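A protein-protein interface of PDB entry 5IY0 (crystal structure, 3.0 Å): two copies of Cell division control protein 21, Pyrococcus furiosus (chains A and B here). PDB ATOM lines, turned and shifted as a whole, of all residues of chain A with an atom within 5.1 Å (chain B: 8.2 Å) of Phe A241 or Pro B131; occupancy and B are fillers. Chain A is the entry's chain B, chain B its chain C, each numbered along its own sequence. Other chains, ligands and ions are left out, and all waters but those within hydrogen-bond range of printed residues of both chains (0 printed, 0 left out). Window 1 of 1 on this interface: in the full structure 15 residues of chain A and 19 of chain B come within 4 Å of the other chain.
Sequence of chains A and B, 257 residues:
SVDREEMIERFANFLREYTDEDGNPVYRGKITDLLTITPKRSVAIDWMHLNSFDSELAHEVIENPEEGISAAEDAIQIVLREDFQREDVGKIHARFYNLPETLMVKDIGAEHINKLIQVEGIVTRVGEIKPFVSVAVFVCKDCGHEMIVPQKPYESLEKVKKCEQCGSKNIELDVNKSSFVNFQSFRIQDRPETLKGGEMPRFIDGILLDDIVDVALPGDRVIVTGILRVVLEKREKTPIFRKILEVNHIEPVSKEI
The backbone NH (N) of Phe A241 is in hydrogen-bond range of the backbone carbonyl oxygen (O) of Pro B131. The backbone carbonyl oxygen (O) of Pro A239 lies within hydrogen-bond range of the backbone NH (N) of Val B133, at 3.0 Å. O of Ile B129 is in hydrogen-bond range of NZ of Lys A243, at 2.9 Å. The side-chain amide oxygen (OD1) of Asn B182 is in hydrogen-bond range of the backbone NH (N) of Ala A110 (2.8 Å). The side-chain amino group (NZ) of Lys B130 lies within salt-bridge range of the side-chain carboxylate (OE1) of Glu A233, 3.1 Å away.
O of Ile A240 sits close to N of Glu A233, at 3.3 Å. O of Val B181 sits at hydrogen-bond distance from N of Phe B132, at 2.9 Å. The backbone carbonyl oxygen (O) of Lys B130 is in hydrogen-bond range of the backbone NH (N) of Phe B183, at 2.8 Å.
Among the printed residues, pairs that only touch across the chains: Pro A239 with Phe B132, Phe A241 with Lys B130, Ile A240 with Pro B131, Ile A240 with Lys B130, Leu A232 with Leu B157, Ile A113 with Phe B180, Phe A241 with Val B133, Phe A241 with Phe B180, Ile A113 with Val B175, Ile A240 with Phe B183, Ala A110 with Val B181, Pro A239 with Pro B131, Phe A241 with Leu B173, Val A230 with Pro B131, Val A230 with Phe B180 and Lys A243 with Pro B131.
Of chain B, only Lys B130, Pro B131, Val B133, Leu B173 and Phe B180 come within 4 Å of Phe A241. Of the printed residues of chain A, Pro B131 touches Val A230, Pro A239, Ile A240, Phe A241 and Lys A243. Of the printed residues of chain A, Phe B180 touches Ile A113 (3.5 Å), Val A230 (3.99 Å) and Phe A241 (3.8 Å). Of the printed residues of chain B, Leu A232 touches Leu B157. The nearest printed residue of chain A that does not touch Pro B131 is Ile A113 (4.1 Å).
Of the 20 printed residues of chain B, 12 touch a printed residue of chain A. Hydrophobic or aromatic side chains of chain B that line the printed part of chain A: Pro B131, Phe B132, Val B133, Leu B157, Leu B173, Val B175, Phe B180 and Phe B183. Of the 11 printed residues of chain A, 9 touch a printed residue of chain B. Hydrophobic or aromatic side chains of chain A within 4 Å of the printed part of chain B: Ala A110, Ile A113, Val A230, Leu A232, Pro A239, Ile A240 and Phe A241. Among the printed residues, Asp or Glu carboxylates within 4 Å of a Lys or Arg side-chain nitrogen of the other chain: Glu A233 with Lys B130 (3.1 Å).
No position is printed for both chains.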
ATOM      1  N   ALA A 110      -8.098   6.946   9.942  1.00  0.00           N
ATOM      2  CA  ALA A 110      -9.385   7.360  10.462  1.00  0.00           C
ATOM      3  C   ALA A 110     -10.437   7.604   9.376  1.00  0.00           C
ATOM      4  O   ALA A 110     -11.643   7.530   9.658  1.00  0.00           O
ATOM      5  CB  ALA A 110      -9.217   8.593  11.329  1.00  0.00           C
ATOM      6  N   ILE A 113     -13.100   4.686   8.984  1.00  0.00           N
ATOM      7  CA  ILE A 113     -13.971   4.241  10.063  1.00  0.00           C
ATOM      8  C   ILE A 113     -15.369   3.912   9.525  1.00  0.00           C
ATOM      9  O   ILE A 113     -15.951   4.650   8.755  1.00  0.00           O
ATOM     10  CB  ILE A 113     -14.030   5.279  11.202  1.00  0.00           C
ATOM     11  CG1 ILE A 113     -12.667   5.343  11.904  1.00  0.00           C
ATOM     12  CG2 ILE A 113     -15.142   4.926  12.179  1.00  0.00           C
ATOM     13  CD1 ILE A 113     -12.514   6.473  12.882  1.00  0.00           C
ATOM     14  N   VAL A 230     -13.814   1.244  15.587  1.00  0.00           N
ATOM     15  CA  VAL A 230     -12.979   1.855  16.621  1.00  0.00           C
ATOM     16  C   VAL A 230     -13.597   1.642  17.985  1.00  0.00           C
ATOM     17  O   VAL A 230     -14.809   1.618  18.120  1.00  0.00           O
ATOM     18  CB  VAL A 230     -12.780   3.357  16.389  1.00  0.00           C
ATOM     19  CG1 VAL A 230     -12.065   3.602  15.062  1.00  0.00           C
ATOM     20  CG2 VAL A 230     -14.106   4.100  16.437  1.00  0.00           C
ATOM     21  N   VAL A 231     -12.750   1.474  18.988  1.00  0.00           N
ATOM     22  CA  VAL A 231     -13.190   1.389  20.378  1.00  0.00           C
ATOM     23  C   VAL A 231     -12.226   2.230  21.194  1.00  0.00           C
ATOM     24  O   VAL A 231     -11.064   2.376  20.813  1.00  0.00           O
ATOM     25  CB  VAL A 231     -13.208  -0.060  20.891  1.00  0.00           C
ATOM     26  CG1 VAL A 231     -14.444  -0.773  20.372  1.00  0.00           C
ATOM     27  CG2 VAL A 231     -11.937  -0.801  20.487  1.00  0.00           C
ATOM     28  N   LEU A 232     -12.686   2.768  22.317  1.00  0.00           N
ATOM     29  CA  LEU A 232     -11.865   3.705  23.086  1.00  0.00           C
ATOM     30  C   LEU A 232     -10.716   2.944  23.701  1.00  0.00           C
ATOM     31  O   LEU A 232     -10.839   1.748  23.935  1.00  0.00           O
ATOM     32  CB  LEU A 232     -12.668   4.385  24.188  1.00  0.00           C
ATOM     33  CG  LEU A 232     -13.811   5.271  23.702  1.00  0.00           C
ATOM     34  CD1 LEU A 232     -15.051   4.461  23.272  1.00  0.00           C
ATOM     35  CD2 LEU A 232     -14.168   6.274  24.786  1.00  0.00           C
ATOM     36  N   GLU A 233      -9.606   3.634  23.962  1.00  0.00           N
ATOM     37  CA  GLU A 233      -8.445   3.018  24.611  1.00  0.00           C
ATOM     38  C   GLU A 233      -8.859   2.408  25.945  1.00  0.00           C
ATOM     39  O   GLU A 233      -9.819   2.864  26.563  1.00  0.00           O
ATOM     40  CB  GLU A 233      -7.353   4.053  24.863  1.00  0.00           C
ATOM     41  CG  GLU A 233      -6.693   4.610  23.610  1.00  0.00           C
ATOM     42  CD  GLU A 233      -5.667   3.672  23.007  1.00  0.00           C
ATOM     43  OE1 GLU A 233      -4.560   4.145  22.674  1.00  0.00           O
ATOM     44  OE2 GLU A 233      -5.971   2.467  22.865  1.00  0.00           O
ATOM     45  N   PRO A 239      -9.530  10.373  24.317  1.00  0.00           N
ATOM     46  CA  PRO A 239     -10.273  10.377  23.078  1.00  0.00           C
ATOM     47  C   PRO A 239      -9.513   9.696  21.944  1.00  0.00           C
ATOM     48  O   PRO A 239      -9.867   9.889  20.787  1.00  0.00           O
ATOM     49  CB  PRO A 239     -10.437  11.871  22.781  1.00  0.00           C
ATOM     50  CG  PRO A 239      -9.599  12.601  23.785  1.00  0.00           C
ATOM     51  CD  PRO A 239      -8.728  11.598  24.444  1.00  0.00           C
ATOM     52  N   ILE A 240      -8.468   8.934  22.272  1.00  0.00           N
ATOM     53  CA  ILE A 240      -7.737   8.142  21.296  1.00  0.00           C
ATOM     54  C   ILE A 240      -8.410   6.784  21.216  1.00  0.00           C
ATOM     55  O   ILE A 240      -9.010   6.336  22.181  1.00  0.00           O
ATOM     56  CB  ILE A 240      -6.251   8.021  21.680  1.00  0.00           C
ATOM     57  CG1 ILE A 240      -5.494   9.293  21.293  1.00  0.00           C
ATOM     58  CG2 ILE A 240      -5.560   6.904  20.926  1.00  0.00           C
ATOM     59  CD1 ILE A 240      -5.747  10.475  22.196  1.00  0.00           C
ATOM     60  N   PHE A 241      -8.344   6.148  20.052  1.00  0.00           N
ATOM     61  CA  PHE A 241      -9.074   4.915  19.803  1.00  0.00           C
ATOM     62  C   PHE A 241      -8.170   3.810  19.304  1.00  0.00           C
ATOM     63  O   PHE A 241      -7.128   4.047  18.710  1.00  0.00           O
ATOM     64  CB  PHE A 241     -10.194   5.167  18.806  1.00  0.00           C
ATOM     65  CG  PHE A 241     -11.368   5.899  19.393  1.00  0.00           C
ATOM     66  CD1 PHE A 241     -11.287   7.241  19.698  1.00  0.00           C
ATOM     67  CD2 PHE A 241     -12.560   5.249  19.633  1.00  0.00           C
ATOM     68  CE1 PHE A 241     -12.366   7.915  20.230  1.00  0.00           C
ATOM     69  CE2 PHE A 241     -13.653   5.930  20.156  1.00  0.00           C
ATOM     70  CZ  PHE A 241     -13.550   7.259  20.460  1.00  0.00           C
ATOM     71  N   ARG A 242      -8.582   2.586  19.588  1.00  0.00           N
ATOM     72  CA  ARG A 242      -7.926   1.386  19.093  1.00  0.00           C
ATOM     73  C   ARG A 242      -8.711   0.933  17.870  1.00  0.00           C
ATOM     74  O   ARG A 242      -9.941   1.010  17.877  1.00  0.00           O
ATOM     75  CB  ARG A 242      -7.942   0.330  20.197  1.00  0.00           C
ATOM     76  CG  ARG A 242      -7.819  -1.114  19.755  1.00  0.00           C
ATOM     77  CD  ARG A 242      -7.733  -2.007  20.990  1.00  0.00           C
ATOM     78  NE  ARG A 242      -8.086  -3.407  20.735  1.00  0.00           N
ATOM     79  CZ  ARG A 242      -7.356  -4.261  20.011  1.00  0.00           C
ATOM     80  NH1 ARG A 242      -7.775  -5.514  19.864  1.00  0.00           N
ATOM     81  NH2 ARG A 242      -6.217  -3.877  19.423  1.00  0.00           N
ATOM     82  N   LYS A 243      -8.028   0.479  16.821  1.00  0.00           N
ATOM     83  CA  LYS A 243      -8.753   0.063  15.616  1.00  0.00           C
ATOM     84  C   LYS A 243      -8.769  -1.427  15.398  1.00  0.00           C
ATOM     85  O   LYS A 243      -7.767  -2.100  15.592  1.00  0.00           O
ATOM     86  CB  LYS A 243      -8.290   0.795  14.350  1.00  0.00           C
ATOM     87  CG  LYS A 243      -6.824   1.139  14.236  1.00  0.00           C
ATOM     88  CD  LYS A 243      -6.618   2.115  13.084  1.00  0.00           C
ATOM     89  CE  LYS A 243      -5.202   2.046  12.521  1.00  0.00           C
ATOM     90  NZ  LYS A 243      -4.170   2.099  13.584  1.00  0.00           N
ATOM     91  N   GLU B 128       2.391   4.825  17.441  1.00  0.00           N
ATOM     92  CA  GLU B 128       1.587   4.274  16.374  1.00  0.00           C
ATOM     93  C   GLU B 128       0.445   5.237  16.149  1.00  0.00           C
ATOM     94  O   GLU B 128       0.132   6.057  17.019  1.00  0.00           O
ATOM     95  CB  GLU B 128       1.134   2.836  16.673  1.00  0.00           C
ATOM     96  CG  GLU B 128       0.109   2.619  17.780  1.00  0.00           C
ATOM     97  CD  GLU B 128      -0.180   1.128  18.016  1.00  0.00           C
ATOM     98  OE1 GLU B 128       0.678   0.409  18.602  1.00  0.00           O
ATOM     99  OE2 GLU B 128      -1.270   0.667  17.599  1.00  0.00           O
ATOM    100  N   ILE B 129      -0.141   5.168  14.962  1.00  0.00           N
ATOM    101  CA  ILE B 129      -1.113   6.155  14.524  1.00  0.00           C
ATOM    102  C   ILE B 129      -2.515   5.678  14.828  1.00  0.00           C
ATOM    103  O   ILE B 129      -2.892   4.596  14.432  1.00  0.00           O
ATOM    104  CB  ILE B 129      -0.965   6.421  13.030  1.00  0.00           C
ATOM    105  CG1 ILE B 129       0.437   6.990  12.767  1.00  0.00           C
ATOM    106  CG2 ILE B 129      -2.050   7.369  12.560  1.00  0.00           C
ATOM    107  CD1 ILE B 129       0.810   7.148  11.313  1.00  0.00           C
ATOM    108  N   LYS B 130      -3.294   6.493  15.519  1.00  0.00           N
ATOM    109  CA  LYS B 130      -4.584   6.053  16.028  1.00  0.00           C
ATOM    110  C   LYS B 130      -5.658   7.090  15.777  1.00  0.00           C
ATOM    111  O   LYS B 130      -5.363   8.266  15.657  1.00  0.00           O
ATOM    112  CB  LYS B 130      -4.478   5.815  17.525  1.00  0.00           C
ATOM    113  CG  LYS B 130      -3.317   4.939  17.966  1.00  0.00           C
ATOM    114  CD  LYS B 130      -3.435   4.687  19.460  1.00  0.00           C
ATOM    115  CE  LYS B 130      -2.207   4.020  20.062  1.00  0.00           C
ATOM    116  NZ  LYS B 130      -1.797   4.701  21.332  1.00  0.00           N
ATOM    117  N   PRO B 131      -6.915   6.666  15.690  1.00  0.00           N
ATOM    118  CA  PRO B 131      -7.995   7.656  15.575  1.00  0.00           C
ATOM    119  C   PRO B 131      -8.214   8.453  16.847  1.00  0.00           C
ATOM    120  O   PRO B 131      -8.145   7.903  17.928  1.00  0.00           O
ATOM    121  CB  PRO B 131      -9.230   6.813  15.256  1.00  0.00           C
ATOM    122  CG  PRO B 131      -8.666   5.577  14.625  1.00  0.00           C
ATOM    123  CD  PRO B 131      -7.379   5.315  15.357  1.00  0.00           C
ATOM    124  N   PHE B 132      -8.458   9.749  16.690  1.00  0.00           N
ATOM    125  CA  PHE B 132      -8.751  10.649  17.781  1.00  0.00           C
ATOM    126  C   PHE B 132     -10.093  11.282  17.474  1.00  0.00           C
ATOM    127  O   PHE B 132     -10.324  11.709  16.360  1.00  0.00           O
ATOM    128  CB  PHE B 132      -7.648  11.702  17.876  1.00  0.00           C
ATOM    129  CG  PHE B 132      -8.067  12.968  18.563  1.00  0.00           C
ATOM    130  CD1 PHE B 132      -8.481  12.957  19.878  1.00  0.00           C
ATOM    131  CD2 PHE B 132      -8.037  14.174  17.900  1.00  0.00           C
ATOM    132  CE1 PHE B 132      -8.869  14.129  20.513  1.00  0.00           C
ATOM    133  CE2 PHE B 132      -8.421  15.349  18.534  1.00  0.00           C
ATOM    134  CZ  PHE B 132      -8.837  15.329  19.844  1.00  0.00           C
ATOM    135  N   VAL B 133     -10.994  11.330  18.441  1.00  0.00           N
ATOM    136  CA  VAL B 133     -12.295  11.956  18.196  1.00  0.00           C
ATOM    137  C   VAL B 133     -12.197  13.455  18.481  1.00  0.00           C
ATOM    138  O   VAL B 133     -12.259  13.884  19.620  1.00  0.00           O
ATOM    139  CB  VAL B 133     -13.434  11.287  19.006  1.00  0.00           C
ATOM    140  CG1 VAL B 133     -13.219  11.332  20.522  1.00  0.00           C
ATOM    141  CG2 VAL B 133     -14.768  11.913  18.650  1.00  0.00           C
ATOM    142  N   SER B 134     -12.010  14.258  17.443  1.00  0.00           N
ATOM    143  CA  SER B 134     -11.843  15.697  17.643  1.00  0.00           C
ATOM    144  C   SER B 134     -13.180  16.348  17.967  1.00  0.00           C
ATOM    145  O   SER B 134     -13.222  17.383  18.619  1.00  0.00           O
ATOM    146  CB  SER B 134     -11.189  16.370  16.426  1.00  0.00           C
ATOM    147  OG  SER B 134     -12.101  16.570  15.369  1.00  0.00           O
ATOM    148  N   ALA B 136     -16.779  14.871  19.463  1.00  0.00           N
ATOM    149  CA  ALA B 136     -17.628  13.789  19.937  1.00  0.00           C
ATOM    150  C   ALA B 136     -19.078  14.241  19.882  1.00  0.00           C
ATOM    151  O   ALA B 136     -19.401  15.354  20.300  1.00  0.00           O
ATOM    152  CB  ALA B 136     -17.254  13.399  21.354  1.00  0.00           C
ATOM    153  N   GLN B 151     -13.179  18.120  21.547  1.00  0.00           N
ATOM    154  CA  GLN B 151     -12.174  17.432  22.365  1.00  0.00           C
ATOM    155  C   GLN B 151     -10.793  17.967  22.109  1.00  0.00           C
ATOM    156  O   GLN B 151     -10.558  18.637  21.118  1.00  0.00           O
ATOM    157  CB  GLN B 151     -12.175  15.957  22.029  1.00  0.00           C
ATOM    158  CG  GLN B 151     -13.521  15.304  22.260  1.00  0.00           C
ATOM    159  CD  GLN B 151     -13.792  15.107  23.719  1.00  0.00           C
ATOM    160  OE1 GLN B 151     -12.854  14.999  24.518  1.00  0.00           O
ATOM    161  NE2 GLN B 151     -15.071  15.040  24.088  1.00  0.00           N
ATOM    162  N   LEU B 157     -11.113  12.460  27.844  1.00  0.00           N
ATOM    163  CA  LEU B 157     -12.363  12.490  27.110  1.00  0.00           C
ATOM    164  C   LEU B 157     -13.418  13.191  27.925  1.00  0.00           C
ATOM    165  O   LEU B 157     -13.755  12.729  29.011  1.00  0.00           O
ATOM    166  CB  LEU B 157     -12.851  11.065  26.772  1.00  0.00           C
ATOM    167  CG  LEU B 157     -14.156  10.969  25.935  1.00  0.00           C
ATOM    168  CD1 LEU B 157     -14.033  11.675  24.593  1.00  0.00           C
ATOM    169  CD2 LEU B 157     -14.621   9.534  25.713  1.00  0.00           C
ATOM    170  N   LEU B 173     -21.771   7.613  23.001  1.00  0.00           N
ATOM    171  CA  LEU B 173     -21.065   8.237  21.889  1.00  0.00           C
ATOM    172  C   LEU B 173     -21.515   7.615  20.566  1.00  0.00           C
ATOM    173  O   LEU B 173     -21.481   6.399  20.415  1.00  0.00           O
ATOM    174  CB  LEU B 173     -19.554   8.056  22.047  1.00  0.00           C
ATOM    175  CG  LEU B 173     -18.696   8.712  20.953  1.00  0.00           C
ATOM    176  CD1 LEU B 173     -18.325  10.126  21.349  1.00  0.00           C
ATOM    177  CD2 LEU B 173     -17.433   7.922  20.668  1.00  0.00           C
ATOM    178  N   VAL B 175     -20.598   7.027  16.926  1.00  0.00           N
ATOM    179  CA  VAL B 175     -19.402   7.063  16.108  1.00  0.00           C
ATOM    180  C   VAL B 175     -19.593   7.727  14.747  1.00  0.00           C
ATOM    181  O   VAL B 175     -18.733   8.501  14.327  1.00  0.00           O
ATOM    182  CB  VAL B 175     -18.815   5.654  15.932  1.00  0.00           C
ATOM    183  CG1 VAL B 175     -17.752   5.632  14.851  1.00  0.00           C
ATOM    184  CG2 VAL B 175     -18.240   5.185  17.256  1.00  0.00           C
ATOM    185  N   SER B 178     -19.948  11.512  15.040  1.00  0.00           N
ATOM    186  CA  SER B 178     -18.729  12.083  15.601  1.00  0.00           C
ATOM    187  C   SER B 178     -17.688  12.262  14.508  1.00  0.00           C
ATOM    188  O   SER B 178     -17.756  11.592  13.494  1.00  0.00           O
ATOM    189  CB  SER B 178     -18.182  11.168  16.680  1.00  0.00           C
ATOM    190  OG  SER B 178     -19.105  11.035  17.727  1.00  0.00           O
ATOM    191  N   SER B 179     -16.725  13.158  14.725  1.00  0.00           N
ATOM    192  CA  SER B 179     -15.660  13.445  13.754  1.00  0.00           C
ATOM    193  C   SER B 179     -14.317  12.973  14.251  1.00  0.00           C
ATOM    194  O   SER B 179     -13.880  13.408  15.323  1.00  0.00           O
ATOM    195  CB  SER B 179     -15.555  14.946  13.524  1.00  0.00           C
ATOM    196  OG  SER B 179     -16.734  15.441  12.924  1.00  0.00           O
ATOM    197  N   PHE B 180     -13.660  12.111  13.471  1.00  0.00           N
ATOM    198  CA  PHE B 180     -12.343  11.558  13.840  1.00  0.00           C
ATOM    199  C   PHE B 180     -11.240  12.040  12.929  1.00  0.00           C
ATOM    200  O   PHE B 180     -11.478  12.369  11.773  1.00  0.00           O
ATOM    201  CB  PHE B 180     -12.342  10.036  13.765  1.00  0.00           C
ATOM    202  CG  PHE B 180     -13.286   9.375  14.724  1.00  0.00           C
ATOM    203  CD1 PHE B 180     -14.653   9.419  14.509  1.00  0.00           C
ATOM    204  CD2 PHE B 180     -12.803   8.680  15.813  1.00  0.00           C
ATOM    205  CE1 PHE B 180     -15.518   8.798  15.371  1.00  0.00           C
ATOM    206  CE2 PHE B 180     -13.673   8.056  16.682  1.00  0.00           C
ATOM    207  CZ  PHE B 180     -15.031   8.117  16.460  1.00  0.00           C
ATOM    208  N   VAL B 181     -10.022  12.062  13.455  1.00  0.00           N
ATOM    209  CA  VAL B 181      -8.820  12.400  12.666  1.00  0.00           C
ATOM    210  C   VAL B 181      -7.666  11.581  13.163  1.00  0.00           C
ATOM    211  O   VAL B 181      -7.686  11.140  14.307  1.00  0.00           O
ATOM    212  CB  VAL B 181      -8.410  13.882  12.775  1.00  0.00           C
ATOM    213  CG1 VAL B 181      -9.545  14.782  12.322  1.00  0.00           C
ATOM    214  CG2 VAL B 181      -7.988  14.211  14.191  1.00  0.00           C
ATOM    215  N   ASN B 182      -6.661  11.384  12.321  1.00  0.00           N
ATOM    216  CA  ASN B 182      -5.487  10.632  12.763  1.00  0.00           C
ATOM    217  C   ASN B 182      -4.645  11.366  13.818  1.00  0.00           C
ATOM    218  O   ASN B 182      -4.590  12.586  13.847  1.00  0.00           O
ATOM    219  CB  ASN B 182      -4.646  10.210  11.566  1.00  0.00           C
ATOM    220  CG  ASN B 182      -5.354   9.185  10.691  1.00  0.00           C
ATOM    221  OD1 ASN B 182      -5.960   8.203  11.179  1.00  0.00           O
ATOM    222  ND2 ASN B 182      -5.269   9.385   9.391  1.00  0.00           N
ATOM    223  N   PHE B 183      -4.022  10.574  14.688  1.00  0.00           N
ATOM    224  CA  PHE B 183      -3.284  11.040  15.865  1.00  0.00           C
ATOM    225  C   PHE B 183      -1.960  10.299  15.933  1.00  0.00           C
ATOM    226  O   PHE B 183      -1.910   9.103  15.716  1.00  0.00           O
ATOM    227  CB  PHE B 183      -4.092  10.682  17.100  1.00  0.00           C
ATOM    228  CG  PHE B 183      -3.377  10.891  18.389  1.00  0.00           C
ATOM    229  CD1 PHE B 183      -3.556  12.048  19.093  1.00  0.00           C
ATOM    230  CD2 PHE B 183      -2.571   9.900  18.931  1.00  0.00           C
ATOM    231  CE1 PHE B 183      -2.919  12.246  20.310  1.00  0.00           C
ATOM    232  CE2 PHE B 183      -1.931  10.082  20.146  1.00  0.00           C
ATOM    233  CZ  PHE B 183      -2.108  11.260  20.840  1.00  0.00           C
ATOM    234  N   GLN B 184      -0.884  10.990  16.249  1.00  0.00           N
ATOM    235  CA  GLN B 184       0.382  10.313  16.423  1.00  0.00           C
ATOM    236  C   GLN B 184       1.228  11.054  17.414  1.00  0.00           C
ATOM    237  O   GLN B 184       1.402  12.272  17.300  1.00  0.00           O
ATOM    238  CB  GLN B 184       1.148  10.203  15.117  1.00  0.00           C
ATOM    239  CG  GLN B 184       2.435   9.426  15.287  1.00  0.00           C
ATOM    240  CD  GLN B 184       3.239   9.261  14.012  1.00  0.00           C
ATOM    241  OE1 GLN B 184       3.272  10.134  13.141  1.00  0.00           O
ATOM    242  NE2 GLN B 184       3.933   8.141  13.917  1.00  0.00           N
ATOM    243  N   LEU B 209      -1.530  15.799  14.652  1.00  0.00           N
ATOM    244  CA  LEU B 209      -2.887  15.473  14.220  1.00  0.00           C
ATOM    245  C   LEU B 209      -3.118  15.632  12.728  1.00  0.00           C
ATOM    246  O   LEU B 209      -2.486  16.452  12.075  1.00  0.00           O
ATOM    247  CB  LEU B 209      -3.918  16.331  14.940  1.00  0.00           C
ATOM    248  CG  LEU B 209      -4.084  16.117  16.434  1.00  0.00           C
ATOM    249  CD1 LEU B 209      -5.259  16.932  16.930  1.00  0.00           C
ATOM    250  CD2 LEU B 209      -4.288  14.646  16.791  1.00  0.00           C
